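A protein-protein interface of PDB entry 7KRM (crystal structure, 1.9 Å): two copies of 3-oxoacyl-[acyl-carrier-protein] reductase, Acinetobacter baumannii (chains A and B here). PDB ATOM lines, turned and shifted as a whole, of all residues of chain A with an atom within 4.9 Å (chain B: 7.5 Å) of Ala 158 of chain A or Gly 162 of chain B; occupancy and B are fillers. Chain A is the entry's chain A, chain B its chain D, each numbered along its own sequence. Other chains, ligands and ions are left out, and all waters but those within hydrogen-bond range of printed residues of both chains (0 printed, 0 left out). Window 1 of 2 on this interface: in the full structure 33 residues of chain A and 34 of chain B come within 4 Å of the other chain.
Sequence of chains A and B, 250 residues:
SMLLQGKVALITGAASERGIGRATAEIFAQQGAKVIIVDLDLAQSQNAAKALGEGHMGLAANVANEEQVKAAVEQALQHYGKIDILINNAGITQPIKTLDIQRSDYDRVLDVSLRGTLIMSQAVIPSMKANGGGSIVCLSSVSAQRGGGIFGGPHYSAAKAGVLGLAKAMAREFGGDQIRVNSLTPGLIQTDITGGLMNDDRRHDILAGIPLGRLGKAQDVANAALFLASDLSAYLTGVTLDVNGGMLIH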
ATOM      1  N   LEU A 110      15.106  20.050 -11.686  1.00  0.00           N
ATOM      2  CA  LEU A 110      15.716  20.750 -10.559  1.00  0.00           C
ATOM      3  C   LEU A 110      16.968  21.513 -10.978  1.00  0.00           C
ATOM      4  O   LEU A 110      17.243  22.593 -10.442  1.00  0.00           O
ATOM      5  CB  LEU A 110      16.054  19.760  -9.444  1.00  0.00           C
ATOM      6  CG  LEU A 110      14.965  19.443  -8.415  1.00  0.00           C
ATOM      7  CD1 LEU A 110      14.675  20.663  -7.548  1.00  0.00           C
ATOM      8  CD2 LEU A 110      13.690  18.941  -9.084  1.00  0.00           C
ATOM      9  N   PRO A 154       4.940  17.073 -10.125  1.00  0.00           N
ATOM     10  CA  PRO A 154       5.359  17.380  -8.746  1.00  0.00           C
ATOM     11  C   PRO A 154       6.813  17.801  -8.616  1.00  0.00           C
ATOM     12  O   PRO A 154       7.135  18.609  -7.737  1.00  0.00           O
ATOM     13  CB  PRO A 154       5.090  16.064  -8.000  1.00  0.00           C
ATOM     14  CG  PRO A 154       4.021  15.393  -8.790  1.00  0.00           C
ATOM     15  CD  PRO A 154       4.254  15.773 -10.224  1.00  0.00           C
ATOM     16  N   HIS A 155       7.711  17.260  -9.443  1.00  0.00           N
ATOM     17  CA  HIS A 155       9.106  17.688  -9.387  1.00  0.00           C
ATOM     18  C   HIS A 155       9.270  19.115  -9.894  1.00  0.00           C
ATOM     19  O   HIS A 155      10.199  19.816  -9.474  1.00  0.00           O
ATOM     20  CB  HIS A 155       9.997  16.724 -10.176  1.00  0.00           C
ATOM     21  CG  HIS A 155       9.640  16.596 -11.626  1.00  0.00           C
ATOM     22  ND1 HIS A 155       8.341  16.637 -12.085  1.00  0.00           N
ATOM     23  CD2 HIS A 155      10.419  16.414 -12.719  1.00  0.00           C
ATOM     24  CE1 HIS A 155       8.335  16.493 -13.398  1.00  0.00           C
ATOM     25  NE2 HIS A 155       9.583  16.356 -13.807  1.00  0.00           N
ATOM     26  N   TYR A 156       8.384  19.565 -10.784  1.00  0.00           N
ATOM     27  CA  TYR A 156       8.374  20.972 -11.168  1.00  0.00           C
ATOM     28  C   TYR A 156       7.848  21.841 -10.032  1.00  0.00           C
ATOM     29  O   TYR A 156       8.429  22.884  -9.716  1.00  0.00           O
ATOM     30  CB  TYR A 156       7.538  21.168 -12.431  1.00  0.00           C
ATOM     31  CG  TYR A 156       7.433  22.607 -12.879  1.00  0.00           C
ATOM     32  CD1 TYR A 156       8.442  23.195 -13.629  1.00  0.00           C
ATOM     33  CD2 TYR A 156       6.325  23.378 -12.553  1.00  0.00           C
ATOM     34  CE1 TYR A 156       8.352  24.509 -14.041  1.00  0.00           C
ATOM     35  CE2 TYR A 156       6.226  24.694 -12.962  1.00  0.00           C
ATOM     36  CZ  TYR A 156       7.243  25.254 -13.705  1.00  0.00           C
ATOM     37  OH  TYR A 156       7.152  26.564 -14.116  1.00  0.00           O
ATOM     38  N   SER A 157       6.745  21.422  -9.401  1.00  0.00           N
ATOM     39  CA  SER A 157       6.250  22.142  -8.231  1.00  0.00           C
ATOM     40  C   SER A 157       7.314  22.209  -7.143  1.00  0.00           C
ATOM     41  O   SER A 157       7.485  23.246  -6.491  1.00  0.00           O
ATOM     42  CB  SER A 157       4.985  21.470  -7.694  1.00  0.00           C
ATOM     43  OG  SER A 157       3.936  21.511  -8.643  1.00  0.00           O
ATOM     44  N   ALA A 158       8.040  21.108  -6.936  1.00  0.00           N
ATOM     45  CA  ALA A 158       9.080  21.080  -5.913  1.00  0.00           C
ATOM     46  C   ALA A 158      10.234  22.008  -6.268  1.00  0.00           C
ATOM     47  O   ALA A 158      10.727  22.750  -5.412  1.00  0.00           O
ATOM     48  CB  ALA A 158       9.591  19.652  -5.727  1.00  0.00           C
ATOM     49  N   ALA A 159      10.683  21.974  -7.524  1.00  0.00           N
ATOM     50  CA  ALA A 159      11.785  22.832  -7.944  1.00  0.00           C
ATOM     51  C   ALA A 159      11.433  24.303  -7.771  1.00  0.00           C
ATOM     52  O   ALA A 159      12.240  25.093  -7.267  1.00  0.00           O
ATOM     53  CB  ALA A 159      12.151  22.537  -9.400  1.00  0.00           C
ATOM     54  N   LYS A 160      10.229  24.694  -8.192  1.00  0.00           N
ATOM     55  CA  LYS A 160       9.839  26.096  -8.096  1.00  0.00           C
ATOM     56  C   LYS A 160       9.576  26.506  -6.652  1.00  0.00           C
ATOM     57  O   LYS A 160       9.777  27.674  -6.299  1.00  0.00           O
ATOM     58  CB  LYS A 160       8.611  26.361  -8.965  1.00  0.00           C
ATOM     59  CG  LYS A 160       8.867  26.246 -10.468  1.00  0.00           C
ATOM     60  CD  LYS A 160      10.082  27.062 -10.901  1.00  0.00           C
ATOM     61  CE  LYS A 160      10.112  27.275 -12.405  1.00  0.00           C
ATOM     62  NZ  LYS A 160      11.266  28.122 -12.812  1.00  0.00           N
ATOM     63  N   ALA A 161       9.133  25.570  -5.807  1.00  0.00           N
ATOM     64  CA  ALA A 161       9.039  25.855  -4.379  1.00  0.00           C
ATOM     65  C   ALA A 161      10.423  26.020  -3.763  1.00  0.00           C
ATOM     66  O   ALA A 161      10.634  26.903  -2.923  1.00  0.00           O
ATOM     67  CB  ALA A 161       8.263  24.748  -3.667  1.00  0.00           C
ATOM     68  N   GLY A 162      11.379  25.180  -4.167  1.00  0.00           N
ATOM     69  CA  GLY A 162      12.746  25.361  -3.708  1.00  0.00           C
ATOM     70  C   GLY A 162      13.309  26.716  -4.090  1.00  0.00           C
ATOM     71  O   GLY A 162      14.058  27.327  -3.324  1.00  0.00           O
ATOM     72  N   LEU B 110      19.892  18.293  -0.608  1.00  0.00           N
ATOM     73  CA  LEU B 110      18.674  18.089  -1.385  1.00  0.00           C
ATOM     74  C   LEU B 110      18.307  16.612  -1.485  1.00  0.00           C
ATOM     75  O   LEU B 110      17.118  16.274  -1.500  1.00  0.00           O
ATOM     76  CB  LEU B 110      18.834  18.687  -2.784  1.00  0.00           C
ATOM     77  CG  LEU B 110      18.506  20.171  -2.980  1.00  0.00           C
ATOM     78  CD1 LEU B 110      17.010  20.414  -2.826  1.00  0.00           C
ATOM     79  CD2 LEU B 110      19.298  21.052  -2.021  1.00  0.00           C
ATOM     80  N   SER B 113      16.433  15.261   1.985  1.00  0.00           N
ATOM     81  CA  SER B 113      15.116  15.835   2.247  1.00  0.00           C
ATOM     82  C   SER B 113      14.197  15.719   1.036  1.00  0.00           C
ATOM     83  O   SER B 113      13.109  15.139   1.122  1.00  0.00           O
ATOM     84  CB  SER B 113      15.259  17.299   2.673  1.00  0.00           C
ATOM     85  OG  SER B 113      15.819  17.393   3.970  1.00  0.00           O
ATOM     86  N   LEU B 114      14.610  16.271  -0.107  1.00  0.00           N
ATOM     87  CA  LEU B 114      13.698  16.362  -1.241  1.00  0.00           C
ATOM     88  C   LEU B 114      13.632  15.050  -2.019  1.00  0.00           C
ATOM     89  O   LEU B 114      12.563  14.440  -2.132  1.00  0.00           O
ATOM     90  CB  LEU B 114      14.107  17.514  -2.162  1.00  0.00           C
ATOM     91  CG  LEU B 114      13.146  17.777  -3.324  1.00  0.00           C
ATOM     92  CD1 LEU B 114      11.725  17.992  -2.821  1.00  0.00           C
ATOM     93  CD2 LEU B 114      13.611  18.971  -4.142  1.00  0.00           C
ATOM     94  N   THR B 117      12.217  12.260   0.141  1.00  0.00           N
ATOM     95  CA  THR B 117      10.769  12.311   0.310  1.00  0.00           C
ATOM     96  C   THR B 117      10.063  11.807  -0.942  1.00  0.00           C
ATOM     97  O   THR B 117       9.050  11.104  -0.853  1.00  0.00           O
ATOM     98  CB  THR B 117      10.323  13.734   0.650  1.00  0.00           C
ATOM     99  OG1 THR B 117      10.822  14.098   1.943  1.00  0.00           O
ATOM    100  CG2 THR B 117       8.806  13.835   0.654  1.00  0.00           C
ATOM    101  N   LEU B 118      10.591  12.141  -2.120  1.00  0.00           N
ATOM    102  CA  LEU B 118       9.994  11.663  -3.362  1.00  0.00           C
ATOM    103  C   LEU B 118      10.116  10.149  -3.480  1.00  0.00           C
ATOM    104  O   LEU B 118       9.127   9.456  -3.742  1.00  0.00           O
ATOM    105  CB  LEU B 118      10.651  12.350  -4.559  1.00  0.00           C
ATOM    106  CG  LEU B 118      10.207  11.872  -5.944  1.00  0.00           C
ATOM    107  CD1 LEU B 118       8.712  12.076  -6.128  1.00  0.00           C
ATOM    108  CD2 LEU B 118      10.990  12.590  -7.037  1.00  0.00           C
ATOM    109  N   SER B 140       9.367  19.737   6.810  1.00  0.00           N
ATOM    110  CA  SER B 140       9.957  20.941   6.243  1.00  0.00           C
ATOM    111  C   SER B 140      10.644  21.717   7.360  1.00  0.00           C
ATOM    112  O   SER B 140      11.196  21.115   8.286  1.00  0.00           O
ATOM    113  CB  SER B 140       8.889  21.781   5.548  1.00  0.00           C
ATOM    114  OG  SER B 140       9.456  22.920   4.932  1.00  0.00           O
ATOM    115  N   ALA B 144      12.358  27.282   5.569  1.00  0.00           N
ATOM    116  CA  ALA B 144      11.779  27.317   4.230  1.00  0.00           C
ATOM    117  C   ALA B 144      10.808  28.475   4.059  1.00  0.00           C
ATOM    118  O   ALA B 144      10.601  28.941   2.932  1.00  0.00           O
ATOM    119  CB  ALA B 144      11.068  25.997   3.934  1.00  0.00           C
ATOM    120  N   TYR B 156      19.639  24.388   2.430  1.00  0.00           N
ATOM    121  CA  TYR B 156      18.710  23.728   3.341  1.00  0.00           C
ATOM    122  C   TYR B 156      17.327  24.368   3.260  1.00  0.00           C
ATOM    123  O   TYR B 156      16.310  23.669   3.189  1.00  0.00           O
ATOM    124  CB  TYR B 156      19.253  23.782   4.769  1.00  0.00           C
ATOM    125  CG  TYR B 156      18.333  23.171   5.803  1.00  0.00           C
ATOM    126  CD1 TYR B 156      18.290  21.796   5.994  1.00  0.00           C
ATOM    127  CD2 TYR B 156      17.514  23.969   6.591  1.00  0.00           C
ATOM    128  CE1 TYR B 156      17.453  21.233   6.937  1.00  0.00           C
ATOM    129  CE2 TYR B 156      16.675  23.414   7.539  1.00  0.00           C
ATOM    130  CZ  TYR B 156      16.648  22.046   7.706  1.00  0.00           C
ATOM    131  OH  TYR B 156      15.815  21.486   8.645  1.00  0.00           O
ATOM    132  N   SER B 157      17.271  25.704   3.273  1.00  0.00           N
ATOM    133  CA  SER B 157      15.994  26.389   3.106  1.00  0.00           C
ATOM    134  C   SER B 157      15.333  25.995   1.792  1.00  0.00           C
ATOM    135  O   SER B 157      14.117  25.783   1.737  1.00  0.00           O
ATOM    136  CB  SER B 157      16.191  27.905   3.160  1.00  0.00           C
ATOM    137  OG  SER B 157      16.757  28.309   4.394  1.00  0.00           O
ATOM    138  N   ALA B 158      16.121  25.899   0.720  1.00  0.00           N
ATOM    139  CA  ALA B 158      15.572  25.511  -0.574  1.00  0.00           C
ATOM    140  C   ALA B 158      15.057  24.079  -0.540  1.00  0.00           C
ATOM    141  O   ALA B 158      13.954  23.793  -1.023  1.00  0.00           O
ATOM    142  CB  ALA B 158      16.635  25.678  -1.659  1.00  0.00           C
ATOM    143  N   ALA B 159      15.843  23.160   0.027  1.00  0.00           N
ATOM    144  CA  ALA B 159      15.424  21.765   0.092  1.00  0.00           C
ATOM    145  C   ALA B 159      14.106  21.624   0.844  1.00  0.00           C
ATOM    146  O   ALA B 159      13.189  20.931   0.387  1.00  0.00           O
ATOM    147  CB  ALA B 159      16.512  20.920   0.758  1.00  0.00           C
ATOM    148  N   LYS B 160      13.996  22.274   2.005  1.00  0.00           N
ATOM    149  CA  LYS B 160      12.786  22.153   2.811  1.00  0.00           C
ATOM    150  C   LYS B 160      11.613  22.891   2.178  1.00  0.00           C
ATOM    151  O   LYS B 160      10.458  22.494   2.372  1.00  0.00           O
ATOM    152  CB  LYS B 160      13.047  22.669   4.228  1.00  0.00           C
ATOM    153  CG  LYS B 160      14.050  21.833   5.025  1.00  0.00           C
ATOM    154  CD  LYS B 160      13.683  20.356   5.011  1.00  0.00           C
ATOM    155  CE  LYS B 160      14.311  19.603   6.173  1.00  0.00           C
ATOM    156  NZ  LYS B 160      13.891  18.176   6.182  1.00  0.00           N
ATOM    157  N   ALA B 161      11.882  23.962   1.429  1.00  0.00           N
ATOM    158  CA  ALA B 161      10.821  24.594   0.650  1.00  0.00           C
ATOM    159  C   ALA B 161      10.384  23.693  -0.497  1.00  0.00           C
ATOM    160  O   ALA B 161       9.190  23.605  -0.807  1.00  0.00           O
ATOM    161  CB  ALA B 161      11.290  25.949   0.121  1.00  0.00           C
ATOM    162  N   GLY B 162      11.338  23.011  -1.134  1.00  0.00           N
ATOM    163  CA  GLY B 162      10.984  22.051  -2.164  1.00  0.00           C
ATOM    164  C   GLY B 162      10.111  20.932  -1.636  1.00  0.00           C
ATOM    165  O   GLY B 162       9.204  20.460  -2.327  1.00  0.00           O
ATOM    166  N   VAL B 163      10.376  20.488  -0.405  1.00  0.00           N
ATOM    167  CA  VAL B 163       9.538  19.468   0.221  1.00  0.00           C
ATOM    168  C   VAL B 163       8.089  19.936   0.280  1.00  0.00           C
ATOM    169  O   VAL B 163       7.161  19.167   0.004  1.00  0.00           O
ATOM    170  CB  VAL B 163      10.078  19.119   1.620  1.00  0.00           C
ATOM    171  CG1 VAL B 163       9.051  18.310   2.406  1.00  0.00           C
ATOM    172  CG2 VAL B 163      11.385  18.350   1.506  1.00  0.00           C
ATOM    173  N   LEU B 164       7.872  21.205   0.640  1.00  0.00           N
ATOM    174  CA  LEU B 164       6.514  21.739   0.709  1.00  0.00           C
ATOM    175  C   LEU B 164       5.834  21.685  -0.653  1.00  0.00           C
ATOM    176  O   LEU B 164       4.672  21.274  -0.765  1.00  0.00           O
ATOM    177  CB  LEU B 164       6.539  23.174   1.235  1.00  0.00           C
ATOM    178  CG  LEU B 164       7.010  23.368   2.676  1.00  0.00           C
ATOM    179  CD1 LEU B 164       7.063  24.853   3.021  1.00  0.00           C
ATOM    180  CD2 LEU B 164       6.105  22.620   3.645  1.00  0.00           C
ATOM    181  N   GLY B 165       6.540  22.110  -1.703  1.00  0.00           N
ATOM    182  CA  GLY B 165       5.966  22.055  -3.038  1.00  0.00           C
ATOM    183  C   GLY B 165       5.635  20.640  -3.469  1.00  0.00           C
ATOM    184  O   GLY B 165       4.574  20.387  -4.044  1.00  0.00           O
ATOM    185  N   LEU B 166       6.540  19.698  -3.196  1.00  0.00           N
ATOM    186  CA  LEU B 166       6.283  18.299  -3.522  1.00  0.00           C
ATOM    187  C   LEU B 166       5.091  17.766  -2.739  1.00  0.00           C
ATOM    188  O   LEU B 166       4.208  17.106  -3.300  1.00  0.00           O
ATOM    189  CB  LEU B 166       7.527  17.460  -3.232  1.00  0.00           C
ATOM    190  CG  LEU B 166       7.401  15.962  -3.518  1.00  0.00           C
ATOM    191  CD1 LEU B 166       7.234  15.714  -5.010  1.00  0.00           C
ATOM    192  CD2 LEU B 166       8.603  15.211  -2.976  1.00  0.00           C
ATOM    193  N   ALA B 167       5.050  18.041  -1.433  1.00  0.00           N
ATOM    194  CA  ALA B 167       3.956  17.546  -0.605  1.00  0.00           C
ATOM    195  C   ALA B 167       2.614  18.082  -1.085  1.00  0.00           C
ATOM    196  O   ALA B 167       1.629  17.338  -1.161  1.00  0.00           O
ATOM    197  CB  ALA B 167       4.193  17.928   0.856  1.00  0.00           C
ATOM    198  N   LYS B 168       2.553  19.374  -1.412  1.00  0.00           N
ATOM    199  CA  LYS B 168       1.304  19.943  -1.910  1.00  0.00           C
ATOM    200  C   LYS B 168       0.902  19.309  -3.234  1.00  0.00           C
ATOM    201  O   LYS B 168      -0.282  19.027  -3.463  1.00  0.00           O
ATOM    202  CB  LYS B 168       1.443  21.454  -2.065  1.00  0.00           C
ATOM    203  CG  LYS B 168       1.663  22.197  -0.759  1.00  0.00           C
ATOM    204  CD  LYS B 168       1.920  23.667  -1.021  1.00  0.00           C
ATOM    205  CE  LYS B 168       2.500  24.366   0.194  1.00  0.00           C
ATOM    206  NZ  LYS B 168       2.782  25.799  -0.096  1.00  0.00           N
ATOM    207  N   ALA B 169       1.872  19.076  -4.122  1.00  0.00           N
ATOM    208  CA  ALA B 169       1.559  18.478  -5.416  1.00  0.00           C
ATOM    209  C   ALA B 169       1.051  17.050  -5.256  1.00  0.00           C
ATOM    210  O   ALA B 169       0.122  16.634  -5.961  1.00  0.00           O
ATOM    211  CB  ALA B 169       2.792  18.507  -6.319  1.00  0.00           C
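Hydrophobic or aromatic side chains of chain A that line the printed part of chain B: Leu 110, Pro 154, Ala 158 and Ala 161. Hydrophobic or aromatic side chains of chain B that line the printed part of chain A: Leu 114, Ala 158, Ala 161, Leu 166 and Ala 169. Among the printed residues, no Asp or Glu carboxylate lies within 4 Å of a Lys or Arg side-chain nitrogen of the other chain.
Ala 158 of chain A touches Gly 162 of chain B, and with the chains exchanged Gly 162 of chain A touches Ala 158 of chain B. Ala 161 of chain A touches its own counterpart, Ala 161 of chain B. Gly 162 of chain A touches its own counterpart, Gly 162 of chain B. Of the 12 pairs that touch across the chains among the printed residues, 4 have their exchanged pair printed and touching as well.
Of chain B, only Leu 114 (3.97 Å), Gly 162 (3.3 Å) and Leu 166 (3.9 Å) come within 4 Å of Ala 158 of chain A. Of chain A, only Ala 158 (3.3 Å) and Gly 162 (3.7 Å) come within 4 Å of Gly 162 of chain B. Of the printed residues of chain A, Leu 114 of chain B touches Leu 110 and Ala 158. Of the printed residues of chain A, Ala 158 of chain B touches Gly 162. Of the printed residues of chain A, Ala 161 of chain B touches Ala 161. Of the printed residues of chain B, Leu 110 of chain A touches Leu 114. Of the printed residues of chain B, Gly 162 of chain A touches Ala 158 (3.3 Å) and Gly 162 (3.7 Å). The nearest residue of chain B that does not touch Ala 158 of chain A is Gly 165 of chain B (4.2 Å). The nearest printed residue of chain A that does not touch Ala 161 of chain B is Gly 162 of chain A (4.1 Å).
Among the printed residues, merely in contact across the chains: Ala 161 of chain A with Ala 161 of chain B (3.2 Å), Ala 158 of chain A with Gly 162 of chain B (3.3 Å), Gly 162 of chain A with Ala 158 of chain B (3.3 Å), Ala 161 of chain A with Gly 165 of chain B (3.6 Å), Pro 154 of chain A with Leu 166 of chain B (3.7 Å), Pro 154 of chain A with Ala 169 of chain B (3.7 Å), Gly 162 of chain A with Gly 162 of chain B (3.7 Å), Ser 157 of chain A with Gly 165 of chain B (3.8 Å), Ala 158 of chain A with Leu 166 of chain B (3.9 Å), Ser 157 of chain A with Ala 169 of chain B (3.9 Å), Leu 110 of chain A with Leu 114 of chain B (3.9 Å) and Ala 158 of chain A with Leu 114 of chain B (3.97 Å).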
